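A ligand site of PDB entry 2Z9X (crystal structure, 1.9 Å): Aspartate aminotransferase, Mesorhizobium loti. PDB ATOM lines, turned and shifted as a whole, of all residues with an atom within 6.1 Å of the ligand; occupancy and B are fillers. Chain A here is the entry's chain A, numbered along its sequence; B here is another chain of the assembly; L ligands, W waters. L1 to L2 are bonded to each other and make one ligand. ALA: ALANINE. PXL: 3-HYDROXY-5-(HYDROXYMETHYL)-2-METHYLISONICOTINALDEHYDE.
The side-chain hydroxyl of Thr 145 is in hydrogen-bond range of an oxygen (O3) of PXL L2 (2.5 Å). The guanidinium group of Arg 344 lies within salt-bridge range of an oxygen (O) of ALA L1, at 2.7 Å. OH of Tyr 94 sits at hydrogen-bond distance from N of ALA L1 (2.7 Å). The side-chain carboxylate (OD1) of Asp 170 sits at hydrogen-bond distance from a nitrogen (N1) of PXL L2 (2.7 Å). The side-chain carboxylate of Glu 67 is in hydrogen-bond range of an oxygen (OP4) of PXL L2 (2.7 Å). The side-chain amino group (NZ) of Lys 196 lies within hydrogen-bond range of an oxygen (OP4) of PXL L2, 3.0 Å away.
The backbone carbonyl oxygen (O) of Thr 145 lies close to the guanidinium group (NH1) of Arg 344 (3.4 Å). The side-chain hydroxyl of Thr 145 lies within hydrogen-bond range of the backbone carbonyl oxygen of His 143 (3.3 Å). The side-chain hydroxyl (OG1) of Thr 145 lies within hydrogen-bond range of the side-chain hydroxyl (OG) of Ser 173 (2.6 Å). The backbone NH of Arg 344 sits at hydrogen-bond distance from the backbone carbonyl oxygen of Ser 332 (2.8 Å). OH of Tyr 94 lies within hydrogen-bond range of NE of Arg 335. The backbone NH (N) of Tyr 94 lies within hydrogen-bond range of the side-chain carboxylate (OD1) of Asp 144, at 3.0 Å. The backbone NH of Val 69 lies within hydrogen-bond range of the side-chain carboxylate of Glu 67, 3.0 Å away. SG of Cys 141 sits close to N of Asp 144 (3.8 Å).
Merely in contact with the ligand: His 143, Thr 247 of chain B, Val 172, Ser 173, Cys 141, Gly 16, Pro 146, Pro 68, Val 69, Arg 335 and Leu 72. The nearest printed residue that does not touch the ligand is Ala 15 (4.6 Å).
Water W1 lies within hydrogen-bond range of O of Ala 15 (2.8 Å) and O3 of PXL L2 (2.8 Å). Water W4 lies within hydrogen-bond range of OG of Ser 332 (2.7 Å), O of Gly 16 (2.8 Å), OXT of ALA L1 (3.1 Å) and NH2 of Arg 344 (3.4 Å). Water W2 bridges the side-chain hydroxyl (OG1) of Thr 247 of chain B (2.8 Å) and the side-chain carboxylate (OE1) of Glu 67 (2.8 Å). Water W5 lies within hydrogen-bond range of OG1 of Thr 247 of chain B (2.9 Å) and NZ of Lys 196 (3.0 Å). Water W3 bridges OD2 of Asp 35 of chain B (2.5 Å) and OG1 of Thr 247 of chain B (2.7 Å).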
ATOM      1  N   ALA A  15     -27.620  13.768   8.690  1.00  0.00           N
ATOM      2  CA  ALA A  15     -26.423  13.144   8.130  1.00  0.00           C
ATOM      3  C   ALA A  15     -25.682  14.050   7.141  1.00  0.00           C
ATOM      4  O   ALA A  15     -24.890  13.584   6.348  1.00  0.00           O
ATOM      5  CB  ALA A  15     -26.807  11.789   7.459  1.00  0.00           C
ATOM      6  N   GLY A  16     -25.968  15.357   7.184  1.00  0.00           N
ATOM      7  CA  GLY A  16     -25.228  16.328   6.366  1.00  0.00           C
ATOM      8  C   GLY A  16     -26.200  17.268   5.662  1.00  0.00           C
ATOM      9  O   GLY A  16     -26.998  16.841   4.840  1.00  0.00           O
ATOM     10  N   PRO A  17     -26.161  18.571   6.008  1.00  0.00           N
ATOM     11  CA  PRO A  17     -25.315  19.185   7.024  1.00  0.00           C
ATOM     12  C   PRO A  17     -25.643  18.661   8.422  1.00  0.00           C
ATOM     13  O   PRO A  17     -26.664  17.982   8.603  1.00  0.00           O
ATOM     14  CB  PRO A  17     -25.676  20.688   6.954  1.00  0.00           C
ATOM     15  CG  PRO A  17     -26.897  20.801   6.175  1.00  0.00           C
ATOM     16  CD  PRO A  17     -27.064  19.548   5.357  1.00  0.00           C
ATOM     17  N   GLU A  67     -18.016  23.844  -0.916  1.00  0.00           N
ATOM     18  CA  GLU A  67     -18.288  22.576  -0.229  1.00  0.00           C
ATOM     19  C   GLU A  67     -17.848  21.395  -1.124  1.00  0.00           C
ATOM     20  O   GLU A  67     -17.577  21.577  -2.333  1.00  0.00           O
ATOM     21  CB  GLU A  67     -19.742  22.508   0.278  1.00  0.00           C
ATOM     22  CG  GLU A  67     -20.799  22.026  -0.702  1.00  0.00           C
ATOM     23  CD  GLU A  67     -21.134  20.543  -0.504  1.00  0.00           C
ATOM     24  OE1 GLU A  67     -21.179  19.831  -1.503  1.00  0.00           O
ATOM     25  OE2 GLU A  67     -21.407  20.086   0.619  1.00  0.00           O
ATOM     26  N   PRO A  68     -17.714  20.198  -0.541  1.00  0.00           N
ATOM     27  CA  PRO A  68     -17.046  19.091  -1.245  1.00  0.00           C
ATOM     28  C   PRO A  68     -17.510  18.661  -2.651  1.00  0.00           C
ATOM     29  O   PRO A  68     -16.708  18.031  -3.335  1.00  0.00           O
ATOM     30  CB  PRO A  68     -17.177  17.915  -0.270  1.00  0.00           C
ATOM     31  CG  PRO A  68     -17.091  18.576   1.066  1.00  0.00           C
ATOM     32  CD  PRO A  68     -18.036  19.805   0.850  1.00  0.00           C
ATOM     33  N   VAL A  69     -18.721  18.985  -3.092  1.00  0.00           N
ATOM     34  CA  VAL A  69     -19.056  18.703  -4.521  1.00  0.00           C
ATOM     35  C   VAL A  69     -18.077  19.439  -5.432  1.00  0.00           C
ATOM     36  O   VAL A  69     -17.828  18.994  -6.551  1.00  0.00           O
ATOM     37  CB  VAL A  69     -20.506  19.037  -4.945  1.00  0.00           C
ATOM     38  CG1 VAL A  69     -21.506  18.100  -4.273  1.00  0.00           C
ATOM     39  CG2 VAL A  69     -20.841  20.532  -4.701  1.00  0.00           C
ATOM     40  N   LEU A  72     -15.020  17.084  -5.709  1.00  0.00           N
ATOM     41  CA  LEU A  72     -15.343  15.942  -6.562  1.00  0.00           C
ATOM     42  C   LEU A  72     -15.333  16.301  -8.040  1.00  0.00           C
ATOM     43  O   LEU A  72     -14.714  15.608  -8.850  1.00  0.00           O
ATOM     44  CB  LEU A  72     -16.685  15.318  -6.158  1.00  0.00           C
ATOM     45  CG  LEU A  72     -16.754  14.749  -4.736  1.00  0.00           C
ATOM     46  CD1 LEU A  72     -18.195  14.383  -4.421  1.00  0.00           C
ATOM     47  CD2 LEU A  72     -15.769  13.558  -4.513  1.00  0.00           C
ATOM     48  N   TYR A  94     -24.053   8.719  -4.436  1.00  0.00           N
ATOM     49  CA  TYR A  94     -22.815   9.470  -4.757  1.00  0.00           C
ATOM     50  C   TYR A  94     -21.859   8.721  -5.684  1.00  0.00           C
ATOM     51  O   TYR A  94     -21.286   9.310  -6.577  1.00  0.00           O
ATOM     52  CB  TYR A  94     -22.102  10.002  -3.504  1.00  0.00           C
ATOM     53  CG  TYR A  94     -22.838  11.211  -2.986  1.00  0.00           C
ATOM     54  CD1 TYR A  94     -22.522  12.497  -3.454  1.00  0.00           C
ATOM     55  CD2 TYR A  94     -23.870  11.057  -2.072  1.00  0.00           C
ATOM     56  CE1 TYR A  94     -23.245  13.620  -2.988  1.00  0.00           C
ATOM     57  CE2 TYR A  94     -24.579  12.142  -1.606  1.00  0.00           C
ATOM     58  CZ  TYR A  94     -24.278  13.412  -2.073  1.00  0.00           C
ATOM     59  OH  TYR A  94     -25.016  14.481  -1.587  1.00  0.00           O
ATOM     60  N   CYS A 141     -16.605   5.777  -3.628  1.00  0.00           N
ATOM     61  CA  CYS A 141     -17.127   6.533  -2.498  1.00  0.00           C
ATOM     62  C   CYS A 141     -16.977   5.651  -1.228  1.00  0.00           C
ATOM     63  O   CYS A 141     -17.426   4.512  -1.232  1.00  0.00           O
ATOM     64  CB  CYS A 141     -18.599   6.870  -2.751  1.00  0.00           C
ATOM     65  SG  CYS A 141     -19.380   7.872  -1.462  1.00  0.00           S
ATOM     66  N   HIS A 143     -18.146   6.342   2.231  1.00  0.00           N
ATOM     67  CA  HIS A 143     -19.444   6.263   2.865  1.00  0.00           C
ATOM     68  C   HIS A 143     -20.460   6.895   1.921  1.00  0.00           C
ATOM     69  O   HIS A 143     -20.494   8.127   1.757  1.00  0.00           O
ATOM     70  CB  HIS A 143     -19.371   6.953   4.244  1.00  0.00           C
ATOM     71  CG  HIS A 143     -20.681   7.093   4.984  1.00  0.00           C
ATOM     72  ND1 HIS A 143     -21.770   6.251   4.799  1.00  0.00           N
ATOM     73  CD2 HIS A 143     -21.045   7.969   5.945  1.00  0.00           C
ATOM     74  CE1 HIS A 143     -22.746   6.634   5.605  1.00  0.00           C
ATOM     75  NE2 HIS A 143     -22.329   7.661   6.310  1.00  0.00           N
ATOM     76  N   ASP A 144     -21.269   6.061   1.266  1.00  0.00           N
ATOM     77  CA  ASP A 144     -22.277   6.606   0.353  1.00  0.00           C
ATOM     78  C   ASP A 144     -23.481   6.970   1.183  1.00  0.00           C
ATOM     79  O   ASP A 144     -24.393   6.161   1.386  1.00  0.00           O
ATOM     80  CB  ASP A 144     -22.606   5.641  -0.776  1.00  0.00           C
ATOM     81  CG  ASP A 144     -23.131   6.352  -2.031  1.00  0.00           C
ATOM     82  OD1 ASP A 144     -23.981   7.255  -1.865  1.00  0.00           O
ATOM     83  OD2 ASP A 144     -22.681   6.029  -3.159  1.00  0.00           O
ATOM     84  N   THR A 145     -23.471   8.211   1.663  1.00  0.00           N
ATOM     85  CA  THR A 145     -24.244   8.626   2.820  1.00  0.00           C
ATOM     86  C   THR A 145     -25.761   8.301   2.724  1.00  0.00           C
ATOM     87  O   THR A 145     -26.356   7.846   3.699  1.00  0.00           O
ATOM     88  CB  THR A 145     -23.955  10.118   3.181  1.00  0.00           C
ATOM     89  OG1 THR A 145     -22.582  10.433   2.889  1.00  0.00           O
ATOM     90  CG2 THR A 145     -24.226  10.358   4.671  1.00  0.00           C
ATOM     91  N   PRO A 146     -26.399   8.573   1.568  1.00  0.00           N
ATOM     92  CA  PRO A 146     -27.848   8.272   1.424  1.00  0.00           C
ATOM     93  C   PRO A 146     -28.221   6.801   1.635  1.00  0.00           C
ATOM     94  O   PRO A 146     -29.400   6.482   1.738  1.00  0.00           O
ATOM     95  CB  PRO A 146     -28.153   8.728  -0.014  1.00  0.00           C
ATOM     96  CG  PRO A 146     -27.100   9.806  -0.297  1.00  0.00           C
ATOM     97  CD  PRO A 146     -25.863   9.281   0.386  1.00  0.00           C
ATOM     98  N   ASP A 170     -14.012   9.627  -2.486  1.00  0.00           N
ATOM     99  CA  ASP A 170     -14.919  10.513  -1.767  1.00  0.00           C
ATOM    100  C   ASP A 170     -15.006   9.989  -0.316  1.00  0.00           C
ATOM    101  O   ASP A 170     -15.649   8.959  -0.060  1.00  0.00           O
ATOM    102  CB  ASP A 170     -16.310  10.458  -2.420  1.00  0.00           C
ATOM    103  CG  ASP A 170     -17.371  11.228  -1.645  1.00  0.00           C
ATOM    104  OD1 ASP A 170     -18.412  11.580  -2.254  1.00  0.00           O
ATOM    105  OD2 ASP A 170     -17.182  11.448  -0.429  1.00  0.00           O
ATOM    106  N   VAL A 172     -15.982  12.209   2.183  1.00  0.00           N
ATOM    107  CA  VAL A 172     -16.627  13.391   2.771  1.00  0.00           C
ATOM    108  C   VAL A 172     -17.339  13.084   4.091  1.00  0.00           C
ATOM    109  O   VAL A 172     -17.279  13.877   5.044  1.00  0.00           O
ATOM    110  CB  VAL A 172     -17.606  14.019   1.761  1.00  0.00           C
ATOM    111  CG1 VAL A 172     -18.537  15.062   2.443  1.00  0.00           C
ATOM    112  CG2 VAL A 172     -16.833  14.630   0.601  1.00  0.00           C
ATOM    113  N   SER A 173     -18.021  11.933   4.140  1.00  0.00           N
ATOM    114  CA  SER A 173     -18.845  11.577   5.300  1.00  0.00           C
ATOM    115  C   SER A 173     -18.260  10.471   6.173  1.00  0.00           C
ATOM    116  O   SER A 173     -18.991   9.890   6.971  1.00  0.00           O
ATOM    117  CB  SER A 173     -20.248  11.200   4.849  1.00  0.00           C
ATOM    118  OG  SER A 173     -20.247  10.153   3.886  1.00  0.00           O
ATOM    119  N   LYS A 196     -19.185  17.191   8.255  1.00  0.00           N
ATOM    120  CA  LYS A 196     -19.754  15.953   8.740  1.00  0.00           C
ATOM    121  C   LYS A 196     -19.103  15.615  10.088  1.00  0.00           C
ATOM    122  O   LYS A 196     -19.414  16.249  11.096  1.00  0.00           O
ATOM    123  CB  LYS A 196     -19.606  14.836   7.689  1.00  0.00           C
ATOM    124  CG  LYS A 196     -20.657  14.950   6.562  1.00  0.00           C
ATOM    125  CD  LYS A 196     -20.315  16.103   5.589  1.00  0.00           C
ATOM    126  CE  LYS A 196     -21.411  16.296   4.532  1.00  0.00           C
ATOM    127  NZ  LYS A 196     -21.092  17.445   3.618  1.00  0.00           N
ATOM    128  N   SER A 332     -32.530  12.975   8.819  1.00  0.00           N
ATOM    129  CA  SER A 332     -32.347  13.144   7.384  1.00  0.00           C
ATOM    130  C   SER A 332     -33.261  12.213   6.581  1.00  0.00           C
ATOM    131  O   SER A 332     -33.538  11.063   6.974  1.00  0.00           O
ATOM    132  CB  SER A 332     -30.904  12.876   6.978  1.00  0.00           C
ATOM    133  OG  SER A 332     -30.063  13.975   7.271  1.00  0.00           O
ATOM    134  N   SER A 333     -33.698  12.721   5.433  1.00  0.00           N
ATOM    135  CA  SER A 333     -34.344  11.906   4.426  1.00  0.00           C
ATOM    136  C   SER A 333     -33.258  11.117   3.711  1.00  0.00           C
ATOM    137  O   SER A 333     -32.053  11.338   3.952  1.00  0.00           O
ATOM    138  CB  SER A 333     -35.071  12.809   3.422  1.00  0.00           C
ATOM    139  OG  SER A 333     -34.160  13.538   2.617  1.00  0.00           O
ATOM    140  N   GLY A 334     -33.666  10.181   2.843  1.00  0.00           N
ATOM    141  CA  GLY A 334     -32.756   9.628   1.848  1.00  0.00           C
ATOM    142  C   GLY A 334     -32.453  10.666   0.781  1.00  0.00           C
ATOM    143  O   GLY A 334     -32.766  11.852   0.939  1.00  0.00           O
ATOM    144  N   ARG A 335     -31.861  10.214  -0.321  1.00  0.00           N
ATOM    145  CA  ARG A 335     -31.506  11.090  -1.450  1.00  0.00           C
ATOM    146  C   ARG A 335     -31.604  10.246  -2.717  1.00  0.00           C
ATOM    147  O   ARG A 335     -31.262   9.069  -2.709  1.00  0.00           O
ATOM    148  CB  ARG A 335     -30.085  11.635  -1.259  1.00  0.00           C
ATOM    149  CG  ARG A 335     -29.629  12.579  -2.347  1.00  0.00           C
ATOM    150  CD  ARG A 335     -28.282  13.202  -2.090  1.00  0.00           C
ATOM    151  NE  ARG A 335     -27.964  14.116  -3.190  1.00  0.00           N
ATOM    152  CZ  ARG A 335     -28.167  15.431  -3.148  1.00  0.00           C
ATOM    153  NH1 ARG A 335     -28.651  15.997  -2.045  1.00  0.00           N
ATOM    154  NH2 ARG A 335     -27.882  16.194  -4.200  1.00  0.00           N
ATOM    155  N   ARG A 344     -32.468   8.557   7.727  1.00  0.00           N
ATOM    156  CA  ARG A 344     -31.075   8.572   8.223  1.00  0.00           C
ATOM    157  C   ARG A 344     -30.938   9.301   9.541  1.00  0.00           C
ATOM    158  O   ARG A 344     -31.461  10.413   9.738  1.00  0.00           O
ATOM    159  CB  ARG A 344     -30.112   9.170   7.185  1.00  0.00           C
ATOM    160  CG  ARG A 344     -29.929   8.310   5.939  1.00  0.00           C
ATOM    161  CD  ARG A 344     -28.993   8.976   4.945  1.00  0.00           C
ATOM    162  NE  ARG A 344     -29.568  10.165   4.293  1.00  0.00           N
ATOM    163  CZ  ARG A 344     -28.873  11.063   3.588  1.00  0.00           C
ATOM    164  NH1 ARG A 344     -27.537  10.979   3.489  1.00  0.00           N
ATOM    165  NH2 ARG A 344     -29.502  12.067   3.009  1.00  0.00           N
ATOM    166  N   TYR B  34     -29.975  21.466   9.657  1.00  0.00           N
ATOM    167  CA  TYR B  34     -30.155  20.661   8.443  1.00  0.00           C
ATOM    168  C   TYR B  34     -30.782  21.562   7.381  1.00  0.00           C
ATOM    169  O   TYR B  34     -31.731  22.305   7.691  1.00  0.00           O
ATOM    170  CB  TYR B  34     -31.149  19.561   8.769  1.00  0.00           C
ATOM    171  CG  TYR B  34     -31.465  18.525   7.688  1.00  0.00           C
ATOM    172  CD1 TYR B  34     -32.770  18.030   7.574  1.00  0.00           C
ATOM    173  CD2 TYR B  34     -30.460  17.975   6.870  1.00  0.00           C
ATOM    174  CE1 TYR B  34     -33.082  17.042   6.669  1.00  0.00           C
ATOM    175  CE2 TYR B  34     -30.790  16.986   5.901  1.00  0.00           C
ATOM    176  CZ  TYR B  34     -32.103  16.534   5.839  1.00  0.00           C
ATOM    177  OH  TYR B  34     -32.481  15.579   4.939  1.00  0.00           O
ATOM    178  N   ASP B  35     -30.316  21.478   6.142  1.00  0.00           N
ATOM    179  CA  ASP B  35     -30.835  22.400   5.101  1.00  0.00           C
ATOM    180  C   ASP B  35     -32.256  22.098   4.672  1.00  0.00           C
ATOM    181  O   ASP B  35     -32.948  22.976   4.112  1.00  0.00           O
ATOM    182  CB  ASP B  35     -29.880  22.547   3.890  1.00  0.00           C
ATOM    183  CG  ASP B  35     -29.444  21.211   3.285  1.00  0.00           C
ATOM    184  OD1 ASP B  35     -29.692  20.156   3.879  1.00  0.00           O
ATOM    185  OD2 ASP B  35     -28.846  21.241   2.184  1.00  0.00           O
ATOM    186  N   THR B 247     -25.310  21.271  -1.043  1.00  0.00           N
ATOM    187  CA  THR B 247     -25.524  21.849   0.290  1.00  0.00           C
ATOM    188  C   THR B 247     -25.132  23.367   0.360  1.00  0.00           C
ATOM    189  O   THR B 247     -23.980  23.736   0.068  1.00  0.00           O
ATOM    190  CB  THR B 247     -24.812  21.005   1.372  1.00  0.00           C
ATOM    191  OG1 THR B 247     -25.185  19.624   1.213  1.00  0.00           O
ATOM    192  CG2 THR B 247     -25.157  21.492   2.779  1.00  0.00           C
HETATM  193  N   ALA L   1     -24.437  14.513   1.064  1.00  0.00           N
HETATM  194  CA  ALA L   1     -25.608  15.031   1.815  1.00  0.00           C
HETATM  195  C   ALA L   1     -26.619  13.881   2.015  1.00  0.00           C
HETATM  196  O   ALA L   1     -26.130  12.712   2.022  1.00  0.00           O
HETATM  197  CB  ALA L   1     -26.218  16.224   1.013  1.00  0.00           C
HETATM  198  OXT ALA L   1     -27.818  14.159   2.215  1.00  0.00           O
HETATM  199  OP4 PXL L   2     -20.977  17.383   0.594  1.00  0.00           O
HETATM  200  C5A PXL L   2     -21.209  16.697  -0.643  1.00  0.00           C
HETATM  201  C5  PXL L   2     -21.189  15.183  -0.327  1.00  0.00           C
HETATM  202  C6  PXL L   2     -20.229  14.409  -0.980  1.00  0.00           C
HETATM  203  N1  PXL L   2     -20.120  13.106  -0.770  1.00  0.00           N
HETATM  204  C2  PXL L   2     -20.934  12.458   0.051  1.00  0.00           C
HETATM  205  C3  PXL L   2     -21.902  13.188   0.754  1.00  0.00           C
HETATM  206  C4  PXL L   2     -22.070  14.562   0.562  1.00  0.00           C
HETATM  207  C4A PXL L   2     -23.186  15.279   1.329  1.00  0.00           C
HETATM  208  O3  PXL L   2     -22.738  12.595   1.602  1.00  0.00           O
HETATM  209  C2A PXL L   2     -20.745  10.939   0.246  1.00  0.00           C
HETATM  210  O   HOH W   1     -23.244  13.845   4.103  1.00  0.00           O
HETATM  211  O   HOH W   2     -23.776  18.843  -1.069  1.00  0.00           O
HETATM  212  O   HOH W   3     -27.826  19.332   0.987  1.00  0.00           O
HETATM  213  O   HOH W   4     -28.471  14.502   5.199  1.00  0.00           O
HETATM  214  O   HOH W   5     -24.037  17.977   3.279  1.00  0.00           O
